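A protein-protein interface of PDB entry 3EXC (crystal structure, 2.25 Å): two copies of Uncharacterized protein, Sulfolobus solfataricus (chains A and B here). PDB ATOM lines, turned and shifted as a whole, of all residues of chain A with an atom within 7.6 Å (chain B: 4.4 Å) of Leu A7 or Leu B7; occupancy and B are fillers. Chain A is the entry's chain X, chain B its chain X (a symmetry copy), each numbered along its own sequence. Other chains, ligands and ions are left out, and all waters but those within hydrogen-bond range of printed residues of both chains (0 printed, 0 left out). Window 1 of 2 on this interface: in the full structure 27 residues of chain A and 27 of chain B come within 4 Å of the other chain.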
ATOM      1  N   LYS A   5     -28.642 -16.275   5.076  1.00  0.00           N
ATOM      2  CA  LYS A   5     -28.427 -16.787   3.736  1.00  0.00           C
ATOM      3  C   LYS A   5     -26.967 -16.839   3.335  1.00  0.00           C
ATOM      4  O   LYS A   5     -26.083 -16.291   3.986  1.00  0.00           O
ATOM      5  CB  LYS A   5     -29.124 -15.900   2.720  1.00  0.00           C
ATOM      6  CG  LYS A   5     -30.491 -15.667   3.071  1.00  0.00           C
ATOM      7  CD  LYS A   5     -31.275 -16.024   1.896  1.00  0.00           C
ATOM      8  CE  LYS A   5     -31.933 -17.351   2.100  1.00  0.00           C
ATOM      9  NZ  LYS A   5     -31.959 -17.884   0.751  1.00  0.00           N
ATOM     10  N   LEU A   6     -26.700 -17.458   2.206  1.00  0.00           N
ATOM     11  CA  LEU A   6     -25.433 -17.223   1.582  1.00  0.00           C
ATOM     12  C   LEU A   6     -25.542 -17.291   0.141  1.00  0.00           C
ATOM     13  O   LEU A   6     -26.468 -17.868  -0.380  1.00  0.00           O
ATOM     14  CB  LEU A   6     -24.347 -18.157   2.110  1.00  0.00           C
ATOM     15  CG  LEU A   6     -24.514 -19.636   2.100  1.00  0.00           C
ATOM     16  CD1 LEU A   6     -24.584 -20.056   0.699  1.00  0.00           C
ATOM     17  CD2 LEU A   6     -23.238 -20.110   2.744  1.00  0.00           C
ATOM     18  N   LEU A   7     -24.614 -16.602  -0.507  1.00  0.00           N
ATOM     19  CA  LEU A   7     -24.455 -16.578  -1.950  1.00  0.00           C
ATOM     20  C   LEU A   7     -23.135 -17.226  -2.266  1.00  0.00           C
ATOM     21  O   LEU A   7     -22.134 -16.973  -1.561  1.00  0.00           O
ATOM     22  CB  LEU A   7     -24.227 -15.175  -2.459  1.00  0.00           C
ATOM     23  CG  LEU A   7     -25.350 -14.225  -2.290  1.00  0.00           C
ATOM     24  CD1 LEU A   7     -24.770 -12.860  -2.764  1.00  0.00           C
ATOM     25  CD2 LEU A   7     -26.380 -14.762  -3.251  1.00  0.00           C
ATOM     26  N   VAL A   8     -23.137 -18.010  -3.327  1.00  0.00           N
ATOM     27  CA  VAL A   8     -21.904 -18.488  -3.884  1.00  0.00           C
ATOM     28  C   VAL A   8     -21.882 -17.936  -5.287  1.00  0.00           C
ATOM     29  O   VAL A   8     -22.788 -18.213  -6.083  1.00  0.00           O
ATOM     30  CB  VAL A   8     -21.934 -19.993  -3.988  1.00  0.00           C
ATOM     31  CG1 VAL A   8     -20.637 -20.489  -4.583  1.00  0.00           C
ATOM     32  CG2 VAL A   8     -22.102 -20.521  -2.598  1.00  0.00           C
ATOM     33  N   VAL A   9     -20.857 -17.178  -5.598  1.00  0.00           N
ATOM     34  CA  VAL A   9     -20.653 -16.615  -6.888  1.00  0.00           C
ATOM     35  C   VAL A   9     -19.331 -17.161  -7.418  1.00  0.00           C
ATOM     36  O   VAL A   9     -18.274 -17.057  -6.785  1.00  0.00           O
ATOM     37  CB  VAL A   9     -20.567 -15.052  -6.739  1.00  0.00           C
ATOM     38  CG1 VAL A   9     -20.372 -14.356  -8.080  1.00  0.00           C
ATOM     39  CG2 VAL A   9     -21.872 -14.545  -6.117  1.00  0.00           C
ATOM     40  N   TYR A  10     -19.322 -17.673  -8.634  1.00  0.00           N
ATOM     41  CA  TYR A  10     -18.064 -18.253  -9.152  1.00  0.00           C
ATOM     42  C   TYR A  10     -17.613 -17.762 -10.571  1.00  0.00           C
ATOM     43  O   TYR A  10     -18.416 -17.277 -11.440  1.00  0.00           O
ATOM     44  CB  TYR A  10     -18.092 -19.789  -9.031  1.00  0.00           C
ATOM     45  CG  TYR A  10     -19.303 -20.445  -9.629  1.00  0.00           C
ATOM     46  CD1 TYR A  10     -20.463 -20.617  -8.887  1.00  0.00           C
ATOM     47  CD2 TYR A  10     -19.302 -20.907 -10.963  1.00  0.00           C
ATOM     48  CE1 TYR A  10     -21.621 -21.206  -9.474  1.00  0.00           C
ATOM     49  CE2 TYR A  10     -20.437 -21.509 -11.541  1.00  0.00           C
ATOM     50  CZ  TYR A  10     -21.585 -21.651 -10.764  1.00  0.00           C
ATOM     51  OH  TYR A  10     -22.716 -22.237 -11.282  1.00  0.00           O
ATOM     52  N   LEU A  30     -28.394 -25.666  -2.530  1.00  0.00           N
ATOM     53  CA  LEU A  30     -28.457 -24.255  -2.980  1.00  0.00           C
ATOM     54  C   LEU A  30     -29.264 -24.164  -4.264  1.00  0.00           C
ATOM     55  O   LEU A  30     -29.374 -25.146  -4.964  1.00  0.00           O
ATOM     56  CB  LEU A  30     -27.094 -23.695  -3.292  1.00  0.00           C
ATOM     57  CG  LEU A  30     -25.968 -23.749  -2.300  1.00  0.00           C
ATOM     58  CD1 LEU A  30     -25.440 -22.357  -2.142  1.00  0.00           C
ATOM     59  CD2 LEU A  30     -26.459 -24.135  -1.026  1.00  0.00           C
ATOM     60  N   GLU A  31     -29.767 -22.978  -4.602  1.00  0.00           N
ATOM     61  CA  GLU A  31     -30.594 -22.796  -5.771  1.00  0.00           C
ATOM     62  C   GLU A  31     -29.954 -21.853  -6.737  1.00  0.00           C
ATOM     63  O   GLU A  31     -29.473 -20.787  -6.329  1.00  0.00           O
ATOM     64  CB  GLU A  31     -31.973 -22.288  -5.349  1.00  0.00           C
ATOM     65  CG  GLU A  31     -32.848 -23.499  -4.928  1.00  0.00           C
ATOM     66  CD  GLU A  31     -34.237 -23.098  -4.519  1.00  0.00           C
ATOM     67  OE1 GLU A  31     -34.735 -22.022  -4.981  1.00  0.00           O
ATOM     68  OE2 GLU A  31     -34.843 -23.862  -3.733  1.00  0.00           O
ATOM     69  N   ILE A  33     -29.507 -18.880  -9.055  1.00  0.00           N
ATOM     70  CA  ILE A  33     -30.169 -17.603  -9.339  1.00  0.00           C
ATOM     71  C   ILE A  33     -29.639 -16.979 -10.641  1.00  0.00           C
ATOM     72  O   ILE A  33     -30.306 -16.121 -11.181  1.00  0.00           O
ATOM     73  CB  ILE A  33     -29.989 -16.565  -8.207  1.00  0.00           C
ATOM     74  CG1 ILE A  33     -28.536 -16.313  -7.981  1.00  0.00           C
ATOM     75  CG2 ILE A  33     -30.609 -17.055  -6.956  1.00  0.00           C
ATOM     76  CD1 ILE A  33     -28.171 -15.064  -7.000  1.00  0.00           C
ATOM     77  N   ALA A  37     -24.091 -18.169 -10.067  1.00  0.00           N
ATOM     78  CA  ALA A  37     -24.401 -17.705  -8.719  1.00  0.00           C
ATOM     79  C   ALA A  37     -25.518 -18.569  -8.192  1.00  0.00           C
ATOM     80  O   ALA A  37     -26.415 -18.950  -8.916  1.00  0.00           O
ATOM     81  CB  ALA A  37     -24.795 -16.221  -8.751  1.00  0.00           C
ATOM     82  N   PHE A  38     -25.425 -18.915  -6.934  1.00  0.00           N
ATOM     83  CA  PHE A  38     -26.420 -19.738  -6.265  1.00  0.00           C
ATOM     84  C   PHE A  38     -26.703 -19.079  -4.919  1.00  0.00           C
ATOM     85  O   PHE A  38     -25.834 -18.332  -4.422  1.00  0.00           O
ATOM     86  CB  PHE A  38     -25.824 -21.125  -5.976  1.00  0.00           C
ATOM     87  CG  PHE A  38     -25.946 -22.088  -7.110  1.00  0.00           C
ATOM     88  CD1 PHE A  38     -26.867 -23.118  -7.047  1.00  0.00           C
ATOM     89  CD2 PHE A  38     -25.134 -21.951  -8.247  1.00  0.00           C
ATOM     90  CE1 PHE A  38     -26.978 -24.039  -8.134  1.00  0.00           C
ATOM     91  CE2 PHE A  38     -25.226 -22.807  -9.349  1.00  0.00           C
ATOM     92  CZ  PHE A  38     -26.138 -23.862  -9.306  1.00  0.00           C
ATOM     93  N   GLU A  39     -27.871 -19.322  -4.337  1.00  0.00           N
ATOM     94  CA  GLU A  39     -28.150 -18.878  -2.945  1.00  0.00           C
ATOM     95  C   GLU A  39     -28.770 -20.018  -2.176  1.00  0.00           C
ATOM     96  O   GLU A  39     -29.328 -20.947  -2.786  1.00  0.00           O
ATOM     97  CB  GLU A  39     -29.069 -17.615  -2.882  1.00  0.00           C
ATOM     98  CG  GLU A  39     -30.374 -17.759  -3.722  1.00  0.00           C
ATOM     99  CD  GLU A  39     -31.552 -18.450  -2.988  1.00  0.00           C
ATOM    100  OE1 GLU A  39     -31.450 -18.557  -1.725  1.00  0.00           O
ATOM    101  OE2 GLU A  39     -32.571 -18.848  -3.672  1.00  0.00           O
ATOM    102  N   GLY A  40     -28.682 -19.992  -0.848  1.00  0.00           N
ATOM    103  CA  GLY A  40     -29.266 -21.074  -0.099  1.00  0.00           C
ATOM    104  C   GLY A  40     -29.277 -20.636   1.333  1.00  0.00           C
ATOM    105  O   GLY A  40     -28.804 -19.557   1.626  1.00  0.00           O
ATOM    106  N   LEU A  50     -19.325 -27.229   2.261  1.00  0.00           N
ATOM    107  CA  LEU A  50     -19.390 -26.274   1.165  1.00  0.00           C
ATOM    108  C   LEU A  50     -17.986 -25.837   0.702  1.00  0.00           C
ATOM    109  O   LEU A  50     -17.650 -25.933  -0.478  1.00  0.00           O
ATOM    110  CB  LEU A  50     -20.255 -25.052   1.521  1.00  0.00           C
ATOM    111  CG  LEU A  50     -20.367 -23.997   0.440  1.00  0.00           C
ATOM    112  CD1 LEU A  50     -20.981 -24.646  -0.748  1.00  0.00           C
ATOM    113  CD2 LEU A  50     -21.251 -22.845   0.911  1.00  0.00           C
ATOM    114  N   VAL A  65     -14.027 -18.059  -6.367  1.00  0.00           N
ATOM    115  CA  VAL A  65     -15.331 -18.322  -5.829  1.00  0.00           C
ATOM    116  C   VAL A  65     -15.492 -17.468  -4.587  1.00  0.00           C
ATOM    117  O   VAL A  65     -14.605 -17.426  -3.719  1.00  0.00           O
ATOM    118  CB  VAL A  65     -15.505 -19.800  -5.455  1.00  0.00           C
ATOM    119  CG1 VAL A  65     -16.954 -20.030  -4.944  1.00  0.00           C
ATOM    120  CG2 VAL A  65     -15.351 -20.721  -6.701  1.00  0.00           C
ATOM    121  N   HIS A  66     -16.609 -16.766  -4.485  1.00  0.00           N
ATOM    122  CA  HIS A  66     -16.902 -16.011  -3.304  1.00  0.00           C
ATOM    123  C   HIS A  66     -18.044 -16.658  -2.567  1.00  0.00           C
ATOM    124  O   HIS A  66     -19.050 -17.028  -3.166  1.00  0.00           O
ATOM    125  CB  HIS A  66     -17.396 -14.688  -3.736  1.00  0.00           C
ATOM    126  CG  HIS A  66     -16.307 -13.734  -3.970  1.00  0.00           C
ATOM    127  ND1 HIS A  66     -15.508 -13.804  -5.091  1.00  0.00           N
ATOM    128  CD2 HIS A  66     -15.821 -12.720  -3.206  1.00  0.00           C
ATOM    129  CE1 HIS A  66     -14.551 -12.886  -4.999  1.00  0.00           C
ATOM    130  NE2 HIS A  66     -14.723 -12.209  -3.872  1.00  0.00           N
ATOM    131  N   ILE A  67     -17.862 -16.896  -1.279  1.00  0.00           N
ATOM    132  CA  ILE A  67     -18.933 -17.441  -0.470  1.00  0.00           C
ATOM    133  C   ILE A  67     -19.236 -16.361   0.544  1.00  0.00           C
ATOM    134  O   ILE A  67     -18.371 -15.990   1.368  1.00  0.00           O
ATOM    135  CB  ILE A  67     -18.512 -18.680   0.260  1.00  0.00           C
ATOM    136  CG1 ILE A  67     -18.072 -19.783  -0.745  1.00  0.00           C
ATOM    137  CG2 ILE A  67     -19.645 -19.103   1.285  1.00  0.00           C
ATOM    138  CD1 ILE A  67     -17.278 -20.925  -0.056  1.00  0.00           C
ATOM    139  N   ILE A  68     -20.438 -15.812   0.413  1.00  0.00           N
ATOM    140  CA  ILE A  68     -20.794 -14.553   1.047  1.00  0.00           C
ATOM    141  C   ILE A  68     -22.035 -14.738   1.912  1.00  0.00           C
ATOM    142  O   ILE A  68     -23.070 -15.088   1.381  1.00  0.00           O
ATOM    143  CB  ILE A  68     -21.136 -13.503   0.000  1.00  0.00           C
ATOM    144  CG1 ILE A  68     -19.901 -13.232  -0.894  1.00  0.00           C
ATOM    145  CG2 ILE A  68     -21.510 -12.167   0.709  1.00  0.00           C
ATOM    146  CD1 ILE A  68     -20.227 -12.492  -2.130  1.00  0.00           C
ATOM    147  N   PRO A  69     -21.927 -14.523   3.249  1.00  0.00           N
ATOM    148  CA  PRO A  69     -23.123 -14.585   4.134  1.00  0.00           C
ATOM    149  C   PRO A  69     -23.954 -13.314   4.005  1.00  0.00           C
ATOM    150  O   PRO A  69     -23.371 -12.246   3.828  1.00  0.00           O
ATOM    151  CB  PRO A  69     -22.506 -14.639   5.557  1.00  0.00           C
ATOM    152  CG  PRO A  69     -21.142 -13.875   5.387  1.00  0.00           C
ATOM    153  CD  PRO A  69     -20.675 -14.194   3.982  1.00  0.00           C
ATOM    154  N   LEU A  70     -25.283 -13.399   4.005  1.00  0.00           N
ATOM    155  CA  LEU A  70     -26.069 -12.208   4.180  1.00  0.00           C
ATOM    156  C   LEU A  70     -27.302 -12.443   4.985  1.00  0.00           C
ATOM    157  O   LEU A  70     -27.655 -13.569   5.185  1.00  0.00           O
ATOM    158  CB  LEU A  70     -26.412 -11.577   2.876  1.00  0.00           C
ATOM    159  CG  LEU A  70     -27.103 -12.375   1.823  1.00  0.00           C
ATOM    160  CD1 LEU A  70     -27.155 -11.412   0.696  1.00  0.00           C
ATOM    161  CD2 LEU A  70     -26.258 -13.530   1.501  1.00  0.00           C
ATOM    162  N   TRP A  75     -31.095 -10.055   1.540  1.00  0.00           N
ATOM    163  CA  TRP A  75     -31.399 -10.822   0.330  1.00  0.00           C
ATOM    164  C   TRP A  75     -32.791 -10.430  -0.246  1.00  0.00           C
ATOM    165  O   TRP A  75     -33.007 -10.191  -1.458  1.00  0.00           O
ATOM    166  CB  TRP A  75     -31.409 -12.278   0.728  1.00  0.00           C
ATOM    167  CG  TRP A  75     -31.919 -13.139  -0.370  1.00  0.00           C
ATOM    168  CD1 TRP A  75     -33.055 -13.912  -0.357  1.00  0.00           C
ATOM    169  CD2 TRP A  75     -31.323 -13.305  -1.661  1.00  0.00           C
ATOM    170  NE1 TRP A  75     -33.195 -14.565  -1.585  1.00  0.00           N
ATOM    171  CE2 TRP A  75     -32.143 -14.212  -2.391  1.00  0.00           C
ATOM    172  CE3 TRP A  75     -30.187 -12.743  -2.288  1.00  0.00           C
ATOM    173  CZ2 TRP A  75     -31.867 -14.570  -3.707  1.00  0.00           C
ATOM    174  CZ3 TRP A  75     -29.890 -13.119  -3.591  1.00  0.00           C
ATOM    175  CH2 TRP A  75     -30.740 -14.006  -4.294  1.00  0.00           C
ATOM    176  N   ARG A  78     -32.933  -7.323  -2.289  1.00  0.00           N
ATOM    177  CA  ARG A  78     -32.196  -7.228  -3.553  1.00  0.00           C
ATOM    178  C   ARG A  78     -33.124  -6.644  -4.643  1.00  0.00           C
ATOM    179  O   ARG A  78     -34.340  -6.631  -4.510  1.00  0.00           O
ATOM    180  CB  ARG A  78     -31.818  -8.655  -3.978  1.00  0.00           C
ATOM    181  CG  ARG A  78     -33.047  -9.463  -4.409  1.00  0.00           C
ATOM    182  CD  ARG A  78     -32.681 -10.944  -4.615  1.00  0.00           C
ATOM    183  NE  ARG A  78     -33.791 -11.788  -4.986  1.00  0.00           N
ATOM    184  CZ  ARG A  78     -34.688 -12.248  -4.106  1.00  0.00           C
ATOM    185  NH1 ARG A  78     -35.657 -13.082  -4.514  1.00  0.00           N
ATOM    186  NH2 ARG A  78     -34.634 -11.858  -2.815  1.00  0.00           N
ATOM    187  N   ILE A  79     -32.517  -6.112  -5.719  1.00  0.00           N
ATOM    188  CA  ILE A  79     -33.178  -5.765  -6.951  1.00  0.00           C
ATOM    189  C   ILE A  79     -32.714  -6.735  -8.031  1.00  0.00           C
ATOM    190  O   ILE A  79     -31.516  -6.915  -8.198  1.00  0.00           O
ATOM    191  CB  ILE A  79     -32.739  -4.387  -7.337  1.00  0.00           C
ATOM    192  CG1 ILE A  79     -33.338  -3.382  -6.360  1.00  0.00           C
ATOM    193  CG2 ILE A  79     -33.240  -4.009  -8.760  1.00  0.00           C
ATOM    194  CD1 ILE A  79     -32.617  -1.991  -6.416  1.00  0.00           C
ATOM    195  N   LEU B   6     -22.719  -3.079  -1.493  1.00  0.00           N
ATOM    196  CA  LEU B   6     -23.540  -3.831  -2.394  1.00  0.00           C
ATOM    197  C   LEU B   6     -22.734  -4.570  -3.341  1.00  0.00           C
ATOM    198  O   LEU B   6     -21.591  -4.244  -3.562  1.00  0.00           O
ATOM    199  CB  LEU B   6     -24.575  -2.955  -3.098  1.00  0.00           C
ATOM    200  CG  LEU B   6     -24.183  -1.737  -3.857  1.00  0.00           C
ATOM    201  CD1 LEU B   6     -23.372  -2.175  -4.994  1.00  0.00           C
ATOM    202  CD2 LEU B   6     -25.513  -1.201  -4.318  1.00  0.00           C
ATOM    203  N   LEU B   7     -23.327  -5.645  -3.836  1.00  0.00           N
ATOM    204  CA  LEU B   7     -22.765  -6.505  -4.863  1.00  0.00           C
ATOM    205  C   LEU B   7     -23.636  -6.376  -6.082  1.00  0.00           C
ATOM    206  O   LEU B   7     -24.879  -6.349  -5.957  1.00  0.00           O
ATOM    207  CB  LEU B   7     -22.943  -7.965  -4.522  1.00  0.00           C
ATOM    208  CG  LEU B   7     -22.219  -8.454  -3.327  1.00  0.00           C
ATOM    209  CD1 LEU B   7     -22.711  -9.921  -3.156  1.00  0.00           C
ATOM    210  CD2 LEU B   7     -20.779  -8.391  -3.769  1.00  0.00           C
ATOM    211  N   VAL B   8     -22.987  -6.339  -7.231  1.00  0.00           N
ATOM    212  CA  VAL B   8     -23.695  -6.470  -8.473  1.00  0.00           C
ATOM    213  C   VAL B   8     -23.121  -7.712  -9.108  1.00  0.00           C
ATOM    214  O   VAL B   8     -21.911  -7.786  -9.352  1.00  0.00           O
ATOM    215  CB  VAL B   8     -23.371  -5.306  -9.376  1.00  0.00           C
ATOM    216  CG1 VAL B   8     -24.111  -5.453 -10.684  1.00  0.00           C
ATOM    217  CG2 VAL B   8     -23.817  -4.067  -8.664  1.00  0.00           C
ATOM    218  N   VAL B   9     -23.974  -8.669  -9.387  1.00  0.00           N
ATOM    219  CA  VAL B   9     -23.613  -9.886 -10.029  1.00  0.00           C
ATOM    220  C   VAL B   9     -24.398  -9.960 -11.335  1.00  0.00           C
ATOM    221  O   VAL B   9     -25.630  -9.862 -11.369  1.00  0.00           O
ATOM    222  CB  VAL B   9     -24.016 -11.081  -9.091  1.00  0.00           C
ATOM    223  CG1 VAL B   9     -23.645 -12.433  -9.688  1.00  0.00           C
ATOM    224  CG2 VAL B   9     -23.284 -10.925  -7.755  1.00  0.00           C
ATOM    225  N   ILE B  33     -14.590  -7.815  -8.436  1.00  0.00           N
ATOM    226  CA  ILE B  33     -14.095  -8.900  -7.584  1.00  0.00           C
ATOM    227  C   ILE B  33     -14.018 -10.226  -8.359  1.00  0.00           C
ATOM    228  O   ILE B  33     -13.324 -11.114  -7.910  1.00  0.00           O
ATOM    229  CB  ILE B  33     -14.972  -9.131  -6.331  1.00  0.00           C
ATOM    230  CG1 ILE B  33     -16.370  -9.447  -6.746  1.00  0.00           C
ATOM    231  CG2 ILE B  33     -14.970  -7.927  -5.471  1.00  0.00           C
ATOM    232  CD1 ILE B  33     -17.367  -9.965  -5.566  1.00  0.00           C
ATOM    233  N   PHE B  38     -19.119  -7.263  -9.032  1.00  0.00           N
ATOM    234  CA  PHE B  38     -18.456  -6.056  -8.565  1.00  0.00           C
ATOM    235  C   PHE B  38     -18.978  -5.784  -7.157  1.00  0.00           C
ATOM    236  O   PHE B  38     -20.088  -6.252  -6.828  1.00  0.00           O
ATOM    237  CB  PHE B  38     -18.879  -4.869  -9.444  1.00  0.00           C
ATOM    238  CG  PHE B  38     -18.063  -4.709 -10.684  1.00  0.00           C
ATOM    239  CD1 PHE B  38     -17.134  -3.689 -10.774  1.00  0.00           C
ATOM    240  CD2 PHE B  38     -18.228  -5.595 -11.760  1.00  0.00           C
ATOM    241  CE1 PHE B  38     -16.358  -3.537 -11.964  1.00  0.00           C
ATOM    242  CE2 PHE B  38     -17.471  -5.508 -12.933  1.00  0.00           C
ATOM    243  CZ  PHE B  38     -16.537  -4.479 -13.055  1.00  0.00           C
ATOM    244  N   GLU B  39     -18.219  -5.066  -6.337  1.00  0.00           N
ATOM    245  CA  GLU B  39     -18.732  -4.595  -5.023  1.00  0.00           C
ATOM    246  C   GLU B  39     -18.387  -3.137  -4.850  1.00  0.00           C
ATOM    247  O   GLU B  39     -17.459  -2.637  -5.509  1.00  0.00           O
ATOM    248  CB  GLU B  39     -18.182  -5.430  -3.821  1.00  0.00           C
ATOM    249  CG  GLU B  39     -16.630  -5.572  -3.826  1.00  0.00           C
ATOM    250  CD  GLU B  39     -15.864  -4.405  -3.152  1.00  0.00           C
ATOM    251  OE1 GLU B  39     -16.549  -3.624  -2.420  1.00  0.00           O
ATOM    252  OE2 GLU B  39     -14.591  -4.302  -3.337  1.00  0.00           O
ATOM    253  N   HIS B  66     -28.227  -9.075 -10.482  1.00  0.00           N
ATOM    254  CA  HIS B  66     -28.675  -8.972  -9.126  1.00  0.00           C
ATOM    255  C   HIS B  66     -27.948  -7.844  -8.443  1.00  0.00           C
ATOM    256  O   HIS B  66     -26.733  -7.716  -8.561  1.00  0.00           O
ATOM    257  CB  HIS B  66     -28.259 -10.205  -8.428  1.00  0.00           C
ATOM    258  CG  HIS B  66     -29.236 -11.288  -8.577  1.00  0.00           C
ATOM    259  ND1 HIS B  66     -29.364 -11.995  -9.754  1.00  0.00           N
ATOM    260  CD2 HIS B  66     -30.193 -11.758  -7.732  1.00  0.00           C
ATOM    261  CE1 HIS B  66     -30.381 -12.844  -9.641  1.00  0.00           C
ATOM    262  NE2 HIS B  66     -30.894 -12.728  -8.423  1.00  0.00           N
ATOM    263  N   ILE B  67     -28.693  -6.956  -7.807  1.00  0.00           N
ATOM    264  CA  ILE B  67     -28.079  -5.882  -7.053  1.00  0.00           C
ATOM    265  C   ILE B  67     -28.491  -6.135  -5.620  1.00  0.00           C
ATOM    266  O   ILE B  67     -29.695  -6.113  -5.283  1.00  0.00           O
ATOM    267  CB  ILE B  67     -28.591  -4.537  -7.470  1.00  0.00           C
ATOM    268  CG1 ILE B  67     -28.297  -4.283  -8.976  1.00  0.00           C
ATOM    269  CG2 ILE B  67     -28.050  -3.430  -6.472  1.00  0.00           C
ATOM    270  CD1 ILE B  67     -29.126  -3.101  -9.548  1.00  0.00           C
ATOM    271  N   ILE B  68     -27.486  -6.454  -4.812  1.00  0.00           N
ATOM    272  CA  ILE B  68     -27.698  -7.058  -3.506  1.00  0.00           C
ATOM    273  C   ILE B  68     -27.025  -6.215  -2.429  1.00  0.00           C
ATOM    274  O   ILE B  68     -25.820  -6.061  -2.476  1.00  0.00           O
ATOM    275  CB  ILE B  68     -27.067  -8.442  -3.446  1.00  0.00           C
ATOM    276  CG1 ILE B  68     -27.736  -9.368  -4.491  1.00  0.00           C
ATOM    277  CG2 ILE B  68     -27.313  -9.061  -2.038  1.00  0.00           C
ATOM    278  CD1 ILE B  68     -26.976 -10.610  -4.739  1.00  0.00           C
ATOM    279  N   LEU B  70     -25.480  -5.584   1.304  1.00  0.00           N
ATOM    280  CA  LEU B  70     -25.087  -6.320   2.476  1.00  0.00           C
ATOM    281  C   LEU B  70     -24.384  -5.472   3.481  1.00  0.00           C
ATOM    282  O   LEU B  70     -23.993  -4.390   3.151  1.00  0.00           O
ATOM    283  CB  LEU B  70     -24.262  -7.509   2.128  1.00  0.00           C
ATOM    284  CG  LEU B  70     -23.025  -7.343   1.313  1.00  0.00           C
ATOM    285  CD1 LEU B  70     -22.589  -8.749   1.130  1.00  0.00           C
ATOM    286  CD2 LEU B  70     -23.402  -6.729   0.035  1.00  0.00           C
ATOM    287  N   TRP B  75     -19.846  -8.723   4.377  1.00  0.00           N
ATOM    288  CA  TRP B  75     -18.869  -8.733   3.286  1.00  0.00           C
ATOM    289  C   TRP B  75     -17.459  -9.146   3.801  1.00  0.00           C
ATOM    290  O   TRP B  75     -16.723  -9.987   3.233  1.00  0.00           O
ATOM    291  CB  TRP B  75     -18.814  -7.329   2.736  1.00  0.00           C
ATOM    292  CG  TRP B  75     -17.700  -7.167   1.767  1.00  0.00           C
ATOM    293  CD1 TRP B  75     -16.605  -6.347   1.893  1.00  0.00           C
ATOM    294  CD2 TRP B  75     -17.555  -7.859   0.522  1.00  0.00           C
ATOM    295  NE1 TRP B  75     -15.779  -6.488   0.775  1.00  0.00           N
ATOM    296  CE2 TRP B  75     -16.347  -7.402  -0.077  1.00  0.00           C
ATOM    297  CE3 TRP B  75     -18.316  -8.854  -0.133  1.00  0.00           C
ATOM    298  CZ2 TRP B  75     -15.883  -7.899  -1.290  1.00  0.00           C
ATOM    299  CZ3 TRP B  75     -17.874  -9.334  -1.359  1.00  0.00           C
ATOM    300  CH2 TRP B  75     -16.657  -8.873  -1.914  1.00  0.00           C
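N of Ile B67 is in hydrogen-bond range of O of Ile A79 (2.9 Å).
Leu B7 touches its own counterpart, Leu A7.
Leu A7 touches Ile B68, and with the chains exchanged Ile A68 touches Leu B7.
Ile A33 touches His B66, and with the chains exchanged His A66 touches Ile B33.
Ile A68 touches Leu B70, and with the chains exchanged Leu A70 touches Ile B68.
Of the 10 pairs that touch across the chains among the printed residues, 7 have their exchanged pair printed and touching as well.
Of the 23 printed residues of chain A, 7 touch a printed residue of chain B.
Hydrophobic or aromatic side chains of chain A that line the printed part of chain B: Leu A7, Ile A33, His A66, Ile A68 and Leu A70.
Among the printed residues, 10 pairs touch across the chains.
Among the printed residues, no Asp or Glu carboxylate lies within 4 Å of a Lys or Arg side-chain nitrogen of the other chain.
Of chain B, only Leu B7 (3.6 Å) and Ile B68 (3.7 Å) come within 4 Å of Leu A7.
Glu A31 touches none of the printed residues of chain B.
Of the printed residues of chain B, Leu A70 touches Ile B68 (3.6 Å).
Trp A75 touches none of the printed residues of chain B.
Printed residues of chain B within 4 Å of Ile A79: His B66 (3.6 Å) and Ile B67 (2.9 Å).
Leu B7 touches just these residues of chain A: Leu A7 and Ile A68.
Printed residues of chain A within 4 Å of His B66: Ile A33 and Ile A79.
Printed residues of chain A within 4 Å of Ile B67: Arg A78 (3.2 Å) and Ile A79 (2.9 Å).
Of the printed residues of chain A, Leu B70 touches Ile A68 (3.6 Å).
The backbone NH (N) of Lys A5 is in hydrogen-bond range of the backbone carbonyl oxygen (O) of Leu A70 (2.9 Å).
O of Leu A7 lies within hydrogen-bond range of N of Ile A68, at 2.8 Å.
O of Val A9 is in hydrogen-bond range of N of His A66 (2.9 Å).
The backbone carbonyl oxygen of Trp A75 is in hydrogen-bond range of the guanidinium group of Arg A78, at 2.7 Å.
The backbone carbonyl oxygen (O) of Leu B7 sits at hydrogen-bond distance from the backbone NH (N) of Ile B68 (2.8 Å).
The backbone carbonyl oxygen of Val B9 is in hydrogen-bond range of the backbone NH of His B66.
Among the printed residues, merely in contact across the chains: Arg A78 with Ile B67 (3.2 Å), Ile A68 with Leu B70 (3.6 Å), Leu A70 with Ile B68 (3.6 Å), Leu A7 with Leu B7 (3.6 Å), Ile A33 with His B66 (3.6 Å), His A66 with Ile B33 (3.6 Å), Ile A79 with His B66 (3.6 Å), Leu A7 with Ile B68 (3.7 Å) and Ile A68 with Leu B7 (3.7 Å).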
